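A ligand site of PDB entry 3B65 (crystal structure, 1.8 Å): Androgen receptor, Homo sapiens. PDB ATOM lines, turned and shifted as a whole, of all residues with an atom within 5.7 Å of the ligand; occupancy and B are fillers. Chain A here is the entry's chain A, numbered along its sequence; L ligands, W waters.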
ATOM      1  N   LEU A  31       3.678 -21.531  37.813  1.00  0.00           N
ATOM      2  CA  LEU A  31       2.781 -21.839  36.699  1.00  0.00           C
ATOM      3  C   LEU A  31       1.348 -22.088  37.171  1.00  0.00           C
ATOM      4  O   LEU A  31       0.391 -21.666  36.503  1.00  0.00           O
ATOM      5  CB  LEU A  31       3.299 -23.049  35.912  1.00  0.00           C
ATOM      6  CG  LEU A  31       3.925 -22.718  34.554  1.00  0.00           C
ATOM      7  CD1 LEU A  31       2.878 -22.079  33.656  1.00  0.00           C
ATOM      8  CD2 LEU A  31       5.116 -21.774  34.734  1.00  0.00           C
ATOM      9  N   LEU A  34      -0.122 -18.785  37.700  1.00  0.00           N
ATOM     10  CA  LEU A  34      -0.370 -18.096  36.444  1.00  0.00           C
ATOM     11  C   LEU A  34      -1.670 -18.661  35.845  1.00  0.00           C
ATOM     12  O   LEU A  34      -2.515 -17.896  35.408  1.00  0.00           O
ATOM     13  CB  LEU A  34       0.791 -18.282  35.464  1.00  0.00           C
ATOM     14  CG  LEU A  34       2.034 -17.421  35.731  1.00  0.00           C
ATOM     15  CD1 LEU A  34       3.154 -17.822  34.774  1.00  0.00           C
ATOM     16  CD2 LEU A  34       1.693 -15.943  35.568  1.00  0.00           C
ATOM     17  N   ASN A  35      -1.806 -19.991  35.847  1.00  0.00           N
ATOM     18  CA  ASN A  35      -3.002 -20.653  35.313  1.00  0.00           C
ATOM     19  C   ASN A  35      -4.256 -20.221  36.066  1.00  0.00           C
ATOM     20  O   ASN A  35      -5.257 -19.866  35.441  1.00  0.00           O
ATOM     21  CB  ASN A  35      -2.883 -22.188  35.399  1.00  0.00           C
ATOM     22  CG  ASN A  35      -1.847 -22.752  34.424  1.00  0.00           C
ATOM     23  OD1 ASN A  35      -1.428 -22.088  33.480  1.00  0.00           O
ATOM     24  ND2 ASN A  35      -1.453 -24.004  34.650  1.00  0.00           N
ATOM     25  N   GLU A  36      -4.210 -20.259  37.389  1.00  0.00           N
ATOM     26  CA  GLU A  36      -5.345 -19.839  38.221  1.00  0.00           C
ATOM     27  C   GLU A  36      -5.666 -18.361  37.955  1.00  0.00           C
ATOM     28  O   GLU A  36      -6.833 -17.990  37.798  1.00  0.00           O
ATOM     29  CB  GLU A  36      -5.014 -20.051  39.696  1.00  0.00           C
ATOM     30  CG  GLU A  36      -6.070 -19.511  40.677  1.00  0.00           C
ATOM     31  CD  GLU A  36      -7.418 -20.211  40.542  1.00  0.00           C
ATOM     32  OE1 GLU A  36      -8.430 -19.618  40.964  1.00  0.00           O
ATOM     33  OE2 GLU A  36      -7.460 -21.353  40.036  1.00  0.00           O
ATOM     34  N   LEU A  37      -4.638 -17.535  37.900  1.00  0.00           N
ATOM     35  CA  LEU A  37      -4.805 -16.113  37.636  1.00  0.00           C
ATOM     36  C   LEU A  37      -5.426 -15.906  36.262  1.00  0.00           C
ATOM     37  O   LEU A  37      -6.335 -15.093  36.098  1.00  0.00           O
ATOM     38  CB  LEU A  37      -3.459 -15.383  37.704  1.00  0.00           C
ATOM     39  CG  LEU A  37      -3.486 -13.883  37.375  1.00  0.00           C
ATOM     40  CD1 LEU A  37      -4.422 -13.143  38.339  1.00  0.00           C
ATOM     41  CD2 LEU A  37      -2.078 -13.319  37.449  1.00  0.00           C
ATOM     42  N   GLY A  38      -4.936 -16.646  35.271  1.00  0.00           N
ATOM     43  CA  GLY A  38      -5.471 -16.534  33.923  1.00  0.00           C
ATOM     44  C   GLY A  38      -6.966 -16.794  33.938  1.00  0.00           C
ATOM     45  O   GLY A  38      -7.750 -16.036  33.358  1.00  0.00           O
ATOM     46  N   GLN A  41      -8.993 -13.999  35.673  1.00  0.00           N
ATOM     47  CA  GLN A  41      -9.127 -12.841  34.801  1.00  0.00           C
ATOM     48  C   GLN A  41     -10.106 -13.083  33.657  1.00  0.00           C
ATOM     49  O   GLN A  41     -10.807 -12.157  33.250  1.00  0.00           O
ATOM     50  CB  GLN A  41      -7.768 -12.425  34.237  1.00  0.00           C
ATOM     51  CG  GLN A  41      -6.845 -11.858  35.301  1.00  0.00           C
ATOM     52  CD  GLN A  41      -5.626 -11.176  34.723  1.00  0.00           C
ATOM     53  OE1 GLN A  41      -4.658 -10.900  35.431  1.00  0.00           O
ATOM     54  NE2 GLN A  41      -5.665 -10.888  33.411  1.00  0.00           N
ATOM     55  N   GLN A  68     -12.333 -15.839  23.516  1.00  0.00           N
ATOM     56  CA  GLN A  68     -11.328 -16.869  23.722  1.00  0.00           C
ATOM     57  C   GLN A  68     -10.042 -16.653  22.906  1.00  0.00           C
ATOM     58  O   GLN A  68      -8.945 -16.885  23.411  1.00  0.00           O
ATOM     59  CB  GLN A  68     -11.932 -18.248  23.426  1.00  0.00           C
ATOM     60  CG  GLN A  68     -13.145 -18.573  24.324  1.00  0.00           C
ATOM     61  CD  GLN A  68     -13.673 -19.984  24.120  1.00  0.00           C
ATOM     62  OE1 GLN A  68     -13.446 -20.594  23.081  1.00  0.00           O
ATOM     63  NE2 GLN A  68     -14.405 -20.484  25.105  1.00  0.00           N
ATOM     64  N   TYR A  69     -10.158 -16.181  21.658  1.00  0.00           N
ATOM     65  CA  TYR A  69      -8.973 -15.931  20.828  1.00  0.00           C
ATOM     66  C   TYR A  69      -8.161 -14.761  21.395  1.00  0.00           C
ATOM     67  O   TYR A  69      -6.925 -14.834  21.502  1.00  0.00           O
ATOM     68  CB  TYR A  69      -9.335 -15.581  19.371  1.00  0.00           C
ATOM     69  CG  TYR A  69     -10.107 -16.622  18.586  1.00  0.00           C
ATOM     70  CD1 TYR A  69      -9.823 -17.986  18.695  1.00  0.00           C
ATOM     71  CD2 TYR A  69     -11.126 -16.233  17.713  1.00  0.00           C
ATOM     72  CE1 TYR A  69     -10.530 -18.931  17.946  1.00  0.00           C
ATOM     73  CE2 TYR A  69     -11.834 -17.165  16.966  1.00  0.00           C
ATOM     74  CZ  TYR A  69     -11.537 -18.515  17.091  1.00  0.00           C
ATOM     75  OH  TYR A  69     -12.257 -19.435  16.355  1.00  0.00           O
ATOM     76  N   TRP A  71      -8.269 -13.540  24.476  1.00  0.00           N
ATOM     77  CA  TRP A  71      -7.935 -13.714  25.880  1.00  0.00           C
ATOM     78  C   TRP A  71      -6.478 -13.397  26.279  1.00  0.00           C
ATOM     79  O   TRP A  71      -6.245 -12.482  27.057  1.00  0.00           O
ATOM     80  CB  TRP A  71      -8.309 -15.144  26.293  1.00  0.00           C
ATOM     81  CG  TRP A  71      -8.100 -15.507  27.732  1.00  0.00           C
ATOM     82  CD1 TRP A  71      -7.859 -14.671  28.779  1.00  0.00           C
ATOM     83  CD2 TRP A  71      -8.143 -16.838  28.271  1.00  0.00           C
ATOM     84  NE1 TRP A  71      -7.742 -15.393  29.954  1.00  0.00           N
ATOM     85  CE2 TRP A  71      -7.915 -16.723  29.671  1.00  0.00           C
ATOM     86  CE3 TRP A  71      -8.348 -18.105  27.713  1.00  0.00           C
ATOM     87  CZ2 TRP A  71      -7.887 -17.830  30.506  1.00  0.00           C
ATOM     88  CZ3 TRP A  71      -8.329 -19.214  28.559  1.00  0.00           C
ATOM     89  CH2 TRP A  71      -8.096 -19.074  29.938  1.00  0.00           C
ATOM     90  N   MET A  72      -5.520 -14.133  25.741  1.00  0.00           N
ATOM     91  CA  MET A  72      -4.116 -13.919  26.052  1.00  0.00           C
ATOM     92  C   MET A  72      -3.671 -12.469  25.779  1.00  0.00           C
ATOM     93  O   MET A  72      -3.124 -11.797  26.652  1.00  0.00           O
ATOM     94  CB  MET A  72      -3.254 -14.891  25.240  1.00  0.00           C
ATOM     95  CG  MET A  72      -1.766 -14.857  25.578  1.00  0.00           C
ATOM     96  SD  MET A  72      -1.430 -15.436  27.267  1.00  0.00           S
ATOM     97  CE  MET A  72      -1.322 -17.212  27.011  1.00  0.00           C
ATOM     98  N   MET A  75      -4.872  -9.879  28.298  1.00  0.00           N
ATOM     99  CA  MET A  75      -4.171  -9.939  29.582  1.00  0.00           C
ATOM    100  C   MET A  75      -2.783  -9.329  29.481  1.00  0.00           C
ATOM    101  O   MET A  75      -2.341  -8.621  30.387  1.00  0.00           O
ATOM    102  CB  MET A  75      -4.065 -11.380  30.086  1.00  0.00           C
ATOM    103  CG  MET A  75      -5.399 -12.003  30.414  1.00  0.00           C
ATOM    104  SD  MET A  75      -5.233 -13.518  31.375  1.00  0.00           S
ATOM    105  CE  MET A  75      -4.366 -14.546  30.237  1.00  0.00           C
ATOM    106  N   VAL A  76      -2.108  -9.593  28.373  1.00  0.00           N
ATOM    107  CA  VAL A  76      -0.774  -9.071  28.115  1.00  0.00           C
ATOM    108  C   VAL A  76      -0.811  -7.553  28.130  1.00  0.00           C
ATOM    109  O   VAL A  76      -0.035  -6.903  28.835  1.00  0.00           O
ATOM    110  CB  VAL A  76      -0.260  -9.527  26.728  1.00  0.00           C
ATOM    111  CG1 VAL A  76       0.941  -8.693  26.310  1.00  0.00           C
ATOM    112  CG2 VAL A  76       0.110 -11.010  26.766  1.00  0.00           C
ATOM    113  N   ALA A  78      -3.156  -5.440  29.286  1.00  0.00           N
ATOM    114  CA  ALA A  78      -3.567  -4.920  30.587  1.00  0.00           C
ATOM    115  C   ALA A  78      -2.454  -5.053  31.623  1.00  0.00           C
ATOM    116  O   ALA A  78      -2.289  -4.191  32.493  1.00  0.00           O
ATOM    117  CB  ALA A  78      -4.836  -5.648  31.073  1.00  0.00           C
ATOM    118  N   MET A  79      -1.666  -6.121  31.524  1.00  0.00           N
ATOM    119  CA  MET A  79      -0.578  -6.346  32.472  1.00  0.00           C
ATOM    120  C   MET A  79       0.574  -5.353  32.243  1.00  0.00           C
ATOM    121  O   MET A  79       1.207  -4.910  33.196  1.00  0.00           O
ATOM    122  CB  MET A  79      -0.079  -7.797  32.342  1.00  0.00           C
ATOM    123  CG  MET A  79       0.867  -8.263  33.452  1.00  0.00           C
ATOM    124  SD  MET A  79       2.581  -7.748  33.214  1.00  0.00           S
ATOM    125  CE  MET A  79       3.118  -8.958  32.004  1.00  0.00           C
ATOM    126  N   ARG A  82      -0.458  -2.010  33.826  1.00  0.00           N
ATOM    127  CA  ARG A  82      -0.374  -2.101  35.279  1.00  0.00           C
ATOM    128  C   ARG A  82       1.087  -2.086  35.699  1.00  0.00           C
ATOM    129  O   ARG A  82       1.438  -1.478  36.706  1.00  0.00           O
ATOM    130  CB  ARG A  82      -0.997  -3.392  35.825  1.00  0.00           C
ATOM    131  CG  ARG A  82      -2.492  -3.478  35.745  1.00  0.00           C
ATOM    132  CD  ARG A  82      -2.996  -4.611  36.653  1.00  0.00           C
ATOM    133  NE  ARG A  82      -2.481  -5.925  36.271  1.00  0.00           N
ATOM    134  CZ  ARG A  82      -3.001  -6.708  35.329  1.00  0.00           C
ATOM    135  NH1 ARG A  82      -4.068  -6.324  34.643  1.00  0.00           N
ATOM    136  NH2 ARG A  82      -2.456  -7.891  35.089  1.00  0.00           N
ATOM    137  N   TYR A  93       3.686  -6.717  36.731  1.00  0.00           N
ATOM    138  CA  TYR A  93       2.587  -6.737  37.690  1.00  0.00           C
ATOM    139  C   TYR A  93       1.439  -7.629  37.217  1.00  0.00           C
ATOM    140  O   TYR A  93       0.388  -7.131  36.797  1.00  0.00           O
ATOM    141  CB  TYR A  93       2.084  -5.309  37.893  1.00  0.00           C
ATOM    142  CG  TYR A  93       1.420  -5.048  39.227  1.00  0.00           C
ATOM    143  CD1 TYR A  93       2.174  -4.645  40.327  1.00  0.00           C
ATOM    144  CD2 TYR A  93       0.048  -5.182  39.376  1.00  0.00           C
ATOM    145  CE1 TYR A  93       1.560  -4.389  41.557  1.00  0.00           C
ATOM    146  CE2 TYR A  93      -0.574  -4.926  40.598  1.00  0.00           C
ATOM    147  CZ  TYR A  93       0.189  -4.527  41.676  1.00  0.00           C
ATOM    148  OH  TYR A  93      -0.442  -4.232  42.867  1.00  0.00           O
ATOM    149  N   PHE A  94       1.622  -8.954  37.272  1.00  0.00           N
ATOM    150  CA  PHE A  94       0.562  -9.866  36.854  1.00  0.00           C
ATOM    151  C   PHE A  94      -0.638  -9.677  37.774  1.00  0.00           C
ATOM    152  O   PHE A  94      -1.796  -9.688  37.338  1.00  0.00           O
ATOM    153  CB  PHE A  94       1.018 -11.313  36.906  1.00  0.00           C
ATOM    154  CG  PHE A  94       1.999 -11.686  35.833  1.00  0.00           C
ATOM    155  CD1 PHE A  94       3.374 -11.661  36.085  1.00  0.00           C
ATOM    156  CD2 PHE A  94       1.564 -12.103  34.576  1.00  0.00           C
ATOM    157  CE1 PHE A  94       4.296 -12.051  35.112  1.00  0.00           C
ATOM    158  CE2 PHE A  94       2.472 -12.493  33.588  1.00  0.00           C
ATOM    159  CZ  PHE A  94       3.838 -12.464  33.863  1.00  0.00           C
ATOM    160  N   MET A 110       9.546 -18.568  30.980  1.00  0.00           N
ATOM    161  CA  MET A 110       8.904 -17.698  29.985  1.00  0.00           C
ATOM    162  C   MET A 110       9.664 -16.383  29.975  1.00  0.00           C
ATOM    163  O   MET A 110       9.054 -15.324  29.803  1.00  0.00           O
ATOM    164  CB  MET A 110       7.458 -17.396  30.378  1.00  0.00           C
ATOM    165  CG  MET A 110       6.522 -18.561  30.352  1.00  0.00           C
ATOM    166  SD  MET A 110       5.145 -18.238  31.447  1.00  0.00           S
ATOM    167  CE  MET A 110       4.313 -16.968  30.600  1.00  0.00           C
ATOM    168  N   MET A 117       7.243  -8.223  27.368  1.00  0.00           N
ATOM    169  CA  MET A 117       6.138  -7.537  28.022  1.00  0.00           C
ATOM    170  C   MET A 117       6.651  -6.378  28.864  1.00  0.00           C
ATOM    171  O   MET A 117       5.959  -5.374  29.037  1.00  0.00           O
ATOM    172  CB  MET A 117       5.350  -8.515  28.887  1.00  0.00           C
ATOM    173  CG  MET A 117       4.660  -9.594  28.064  1.00  0.00           C
ATOM    174  SD  MET A 117       3.516 -10.629  28.981  1.00  0.00           S
ATOM    175  CE  MET A 117       4.656 -11.950  29.611  1.00  0.00           C
ATOM    176  N   LEU A 203       3.393 -16.762  24.030  1.00  0.00           N
ATOM    177  CA  LEU A 203       2.761 -17.277  25.239  1.00  0.00           C
ATOM    178  C   LEU A 203       1.847 -18.455  24.842  1.00  0.00           C
ATOM    179  O   LEU A 203       1.769 -19.472  25.546  1.00  0.00           O
ATOM    180  CB  LEU A 203       1.953 -16.171  25.930  1.00  0.00           C
ATOM    181  CG  LEU A 203       2.807 -15.097  26.622  1.00  0.00           C
ATOM    182  CD1 LEU A 203       1.930 -13.949  27.129  1.00  0.00           C
ATOM    183  CD2 LEU A 203       3.558 -15.745  27.779  1.00  0.00           C
ATOM    184  N   HIS A 204       1.177 -18.309  23.710  1.00  0.00           N
ATOM    185  CA  HIS A 204       0.299 -19.366  23.224  1.00  0.00           C
ATOM    186  C   HIS A 204       1.127 -20.620  22.972  1.00  0.00           C
ATOM    187  O   HIS A 204       0.802 -21.690  23.482  1.00  0.00           O
ATOM    188  CB  HIS A 204      -0.383 -18.938  21.926  1.00  0.00           C
ATOM    189  CG  HIS A 204      -1.647 -18.162  22.149  1.00  0.00           C
ATOM    190  ND1 HIS A 204      -2.055 -17.142  21.304  1.00  0.00           N
ATOM    191  CD2 HIS A 204      -2.607 -18.273  23.096  1.00  0.00           C
ATOM    192  CE1 HIS A 204      -3.200 -16.663  21.728  1.00  0.00           C
ATOM    193  NE2 HIS A 204      -3.563 -17.323  22.812  1.00  0.00           N
ATOM    194  N   PHE A 206       4.136 -21.429  24.036  1.00  0.00           N
ATOM    195  CA  PHE A 206       4.650 -21.920  25.301  1.00  0.00           C
ATOM    196  C   PHE A 206       3.592 -22.690  26.097  1.00  0.00           C
ATOM    197  O   PHE A 206       3.835 -23.804  26.557  1.00  0.00           O
ATOM    198  CB  PHE A 206       5.181 -20.760  26.141  1.00  0.00           C
ATOM    199  CG  PHE A 206       5.413 -21.101  27.599  1.00  0.00           C
ATOM    200  CD1 PHE A 206       4.381 -20.989  28.522  1.00  0.00           C
ATOM    201  CD2 PHE A 206       6.654 -21.546  28.031  1.00  0.00           C
ATOM    202  CE1 PHE A 206       4.589 -21.327  29.864  1.00  0.00           C
ATOM    203  CE2 PHE A 206       6.872 -21.882  29.364  1.00  0.00           C
ATOM    204  CZ  PHE A 206       5.841 -21.769  30.287  1.00  0.00           C
ATOM    205  N   THR A 207       2.409 -22.096  26.240  1.00  0.00           N
ATOM    206  CA  THR A 207       1.332 -22.719  26.987  1.00  0.00           C
ATOM    207  C   THR A 207       0.880 -24.025  26.361  1.00  0.00           C
ATOM    208  O   THR A 207       0.528 -24.976  27.054  1.00  0.00           O
ATOM    209  CB  THR A 207       0.112 -21.781  27.085  1.00  0.00           C
ATOM    210  OG1 THR A 207       0.504 -20.533  27.657  1.00  0.00           O
ATOM    211  CG2 THR A 207      -0.971 -22.404  27.949  1.00  0.00           C
ATOM    212  N   LEU A 210       3.443 -26.721  27.079  1.00  0.00           N
ATOM    213  CA  LEU A 210       3.353 -27.020  28.502  1.00  0.00           C
ATOM    214  C   LEU A 210       2.179 -27.949  28.837  1.00  0.00           C
ATOM    215  O   LEU A 210       2.329 -28.856  29.656  1.00  0.00           O
ATOM    216  CB  LEU A 210       3.255 -25.718  29.301  1.00  0.00           C
ATOM    217  CG  LEU A 210       3.230 -25.836  30.831  1.00  0.00           C
ATOM    218  CD1 LEU A 210       4.248 -26.874  31.304  1.00  0.00           C
ATOM    219  CD2 LEU A 210       3.518 -24.466  31.435  1.00  0.00           C
ATOM    220  N   PHE A 221      -3.457 -27.654  35.210  1.00  0.00           N
ATOM    221  CA  PHE A 221      -4.212 -26.819  34.296  1.00  0.00           C
ATOM    222  C   PHE A 221      -5.694 -26.861  34.609  1.00  0.00           C
ATOM    223  O   PHE A 221      -6.298 -27.927  34.637  1.00  0.00           O
ATOM    224  CB  PHE A 221      -4.001 -27.234  32.842  1.00  0.00           C
ATOM    225  CG  PHE A 221      -2.772 -26.639  32.226  1.00  0.00           C
ATOM    226  CD1 PHE A 221      -1.557 -27.321  32.261  1.00  0.00           C
ATOM    227  CD2 PHE A 221      -2.822 -25.383  31.636  1.00  0.00           C
ATOM    228  CE1 PHE A 221      -0.406 -26.756  31.721  1.00  0.00           C
ATOM    229  CE2 PHE A 221      -1.667 -24.811  31.092  1.00  0.00           C
ATOM    230  CZ  PHE A 221      -0.456 -25.501  31.131  1.00  0.00           C
ATOM    231  N   MET A 225      -9.347 -23.664  31.008  1.00  0.00           N
ATOM    232  CA  MET A 225      -8.125 -23.324  30.298  1.00  0.00           C
ATOM    233  C   MET A 225      -7.632 -24.501  29.451  1.00  0.00           C
ATOM    234  O   MET A 225      -7.288 -24.314  28.296  1.00  0.00           O
ATOM    235  CB  MET A 225      -7.020 -22.908  31.280  1.00  0.00           C
ATOM    236  CG  MET A 225      -5.818 -22.272  30.592  1.00  0.00           C
ATOM    237  SD  MET A 225      -4.477 -21.810  31.694  1.00  0.00           S
ATOM    238  CE  MET A 225      -5.159 -20.290  32.380  1.00  0.00           C
ATOM    239  N   ILE A 228      -9.661 -24.751  26.301  1.00  0.00           N
ATOM    240  CA  ILE A 228      -9.404 -23.687  25.340  1.00  0.00           C
ATOM    241  C   ILE A 228      -8.033 -23.831  24.687  1.00  0.00           C
ATOM    242  O   ILE A 228      -7.877 -23.532  23.506  1.00  0.00           O
ATOM    243  CB  ILE A 228      -9.544 -22.289  26.012  1.00  0.00           C
ATOM    244  CG1 ILE A 228     -11.017 -22.005  26.292  1.00  0.00           C
ATOM    245  CG2 ILE A 228      -8.958 -21.198  25.108  1.00  0.00           C
ATOM    246  CD1 ILE A 228     -11.271 -20.654  26.950  1.00  0.00           C
ATOM    247  N   ILE A 229      -7.055 -24.299  25.459  1.00  0.00           N
ATOM    248  CA  ILE A 229      -5.708 -24.495  24.925  1.00  0.00           C
ATOM    249  C   ILE A 229      -5.742 -25.579  23.854  1.00  0.00           C
ATOM    250  O   ILE A 229      -5.086 -25.452  22.812  1.00  0.00           O
ATOM    251  CB  ILE A 229      -4.703 -24.925  26.020  1.00  0.00           C
ATOM    252  CG1 ILE A 229      -4.540 -23.824  27.064  1.00  0.00           C
ATOM    253  CG2 ILE A 229      -3.339 -25.224  25.399  1.00  0.00           C
ATOM    254  CD1 ILE A 229      -3.692 -24.215  28.243  1.00  0.00           C
ATOM    255  N   GLN A 232      -9.080 -24.066  21.012  1.00  0.00           N
ATOM    256  CA  GLN A 232      -8.917 -22.779  20.341  1.00  0.00           C
ATOM    257  C   GLN A 232      -7.484 -22.422  19.984  1.00  0.00           C
ATOM    258  O   GLN A 232      -7.196 -22.049  18.843  1.00  0.00           O
ATOM    259  CB  GLN A 232      -9.531 -21.682  21.220  1.00  0.00           C
ATOM    260  CG  GLN A 232     -11.028 -21.880  21.503  1.00  0.00           C
ATOM    261  CD  GLN A 232     -11.897 -21.629  20.273  1.00  0.00           C
ATOM    262  OE1 GLN A 232     -11.645 -22.161  19.196  1.00  0.00           O
ATOM    263  NE2 GLN A 232     -12.932 -20.816  20.441  1.00  0.00           N
ATOM    264  N   VAL A 233      -6.584 -22.539  20.948  1.00  0.00           N
ATOM    265  CA  VAL A 233      -5.181 -22.214  20.717  1.00  0.00           C
ATOM    266  C   VAL A 233      -4.564 -22.892  19.492  1.00  0.00           C
ATOM    267  O   VAL A 233      -3.805 -22.259  18.748  1.00  0.00           O
ATOM    268  CB  VAL A 233      -4.338 -22.513  21.972  1.00  0.00           C
ATOM    269  CG1 VAL A 233      -2.846 -22.279  21.681  1.00  0.00           C
ATOM    270  CG2 VAL A 233      -4.802 -21.626  23.135  1.00  0.00           C
HETATM  271  C1  LIG L   1      -0.738 -14.720  31.615  1.00  0.00           C
HETATM  272  C2  LIG L   1      -0.845 -13.352  31.823  1.00  0.00           C
HETATM  273  I1  LIG L   1       0.096 -12.014  30.506  1.00  0.00           I
HETATM  274  C3  LIG L   1      -1.579 -12.870  32.907  1.00  0.00           C
HETATM  275  C4  LIG L   1      -1.704 -11.475  33.174  1.00  0.00           C
HETATM  276  N1  LIG L   1      -1.795 -10.366  33.404  1.00  0.00           N
HETATM  277  C5  LIG L   1      -2.214 -13.761  33.764  1.00  0.00           C
HETATM  278  C6  LIG L   1      -2.108 -15.134  33.544  1.00  0.00           C
HETATM  279  C7  LIG L   1      -1.377 -15.619  32.476  1.00  0.00           C
HETATM  280  N2  LIG L   1      -1.299 -16.947  32.339  1.00  0.00           N
HETATM  281  C8  LIG L   1      -0.641 -17.603  31.396  1.00  0.00           C
HETATM  282  O1  LIG L   1      -0.001 -17.078  30.486  1.00  0.00           O
HETATM  283  C9  LIG L   1      -0.749 -19.129  31.507  1.00  0.00           C
HETATM  284  O2  LIG L   1      -1.387 -19.468  32.738  1.00  0.00           O
HETATM  285  C10 LIG L   1       0.651 -19.759  31.447  1.00  0.00           C
HETATM  286  C11 LIG L   1      -1.582 -19.646  30.342  1.00  0.00           C
HETATM  287  O3  LIG L   1      -2.890 -19.056  30.396  1.00  0.00           O
HETATM  288  C12 LIG L   1      -3.526 -19.005  29.188  1.00  0.00           C
HETATM  289  C13 LIG L   1      -3.393 -20.007  28.234  1.00  0.00           C
HETATM  290  C14 LIG L   1      -4.098 -19.950  27.038  1.00  0.00           C
HETATM  291  C15 LIG L   1      -4.951 -18.872  26.794  1.00  0.00           C
HETATM  292  C16 LIG L   1      -5.731 -18.843  25.586  1.00  0.00           C
HETATM  293  N3  LIG L   1      -6.349 -18.806  24.640  1.00  0.00           N
HETATM  294  C17 LIG L   1      -5.087 -17.862  27.737  1.00  0.00           C
HETATM  295  C18 LIG L   1      -4.380 -17.933  28.932  1.00  0.00           C
HETATM  296  O   HOH W   1      -4.253  -8.609  32.487  1.00  0.00           O
HETATM  297  O   HOH W   2      -5.981 -16.269  23.661  1.00  0.00           O
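An oxygen (O2) of the ligand is in hydrogen-bond range of the backbone NH (N) of Asn 35. NH2 of Arg 82 is in hydrogen-bond range of N1 of the ligand, 3.1 Å away. The backbone carbonyl oxygen (O) of Leu 34 lies close to an oxygen (O2) of the ligand, at 3.3 Å. The side-chain amide oxygen (OD1) of Asn 35 lies within hydrogen-bond range of an oxygen (O2) of the ligand (2.7 Å).
The guanidinium group of Arg 82 lies within hydrogen-bond range of the backbone carbonyl oxygen of Phe 94, at 3.0 Å. O of Ile 228 lies within hydrogen-bond range of N of Val 233 (3.0 Å). The side-chain amide nitrogen (NE2) of Gln 232 is in hydrogen-bond range of the side-chain amide oxygen (OE1) of Gln 68. The side-chain sulfur (SD) of Met 225 sits close to the side-chain amide oxygen (OD1) of Asn 35 (3.5 Å). The side-chain hydroxyl (OG1) of Thr 207 lies within hydrogen-bond range of the backbone carbonyl oxygen (O) of Leu 203, at 2.7 Å. The side-chain amide nitrogen of Gln 41 sits close to the side-chain sulfur of Met 75 (3.4 Å). O of Gly 38 lies close to NE1 of Trp 71 (3.5 Å). The side-chain sulfur of Met 75 lies within hydrogen-bond range of the indole nitrogen of Trp 71, at 3.4 Å.
The backbone carbonyl oxygen of Gln 68 lies close to a nitrogen (N3) of the ligand (3.5 Å). The side-chain sulfur of Met 225 sits close to an oxygen (O3) of the ligand, 3.4 Å away. CD1 of Leu 31 touches C10 of the ligand, 3.9 Å away. Leu 37 touches the ligand. N of Gly 38 touches C6 of the ligand, at 3.6 Å. Gln 41 touches the ligand. Trp 71 touches the ligand (CD2 to C17, 3.3 Å). Met 72 touches the ligand. Met 75 touches the ligand. Val 76 touches the ligand. CB of Met 79 touches N1 of the ligand (3.3 Å). Phe 94 touches the ligand (CD2 to C4, 3.6 Å). Met 117 touches the ligand (SD to I1, 3.99 Å). His 204 touches the ligand (NE2 to N3, 3.6 Å). CG2 of Thr 207 touches C13 of the ligand, at 3.4 Å. Ile 228 touches the ligand. Ile 229 touches the ligand (CG1 to C14, 3.9 Å). CG2 of Val 233 touches N3 of the ligand, 3.6 Å away. Hydrophobic or aromatic side chains within 4 Å of the ligand: Leu 31, Leu 34, Leu 37, Trp 71, Met 72, Met 75, Val 76, Met 79, Phe 94, Met 117, Met 225, Ile 228, Ile 229 and Val 233. Of the 31 residues printed, 21 come within 4 Å of the ligand. The nearest printed residue that does not touch the ligand is Leu 203 (4.3 Å).
Water W1 lies within hydrogen-bond range of NE2 of Gln 41 (2.8 Å), O of Met 75 (2.8 Å), NH1 of Arg 82 (3.1 Å) and N1 of the ligand (3.2 Å).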
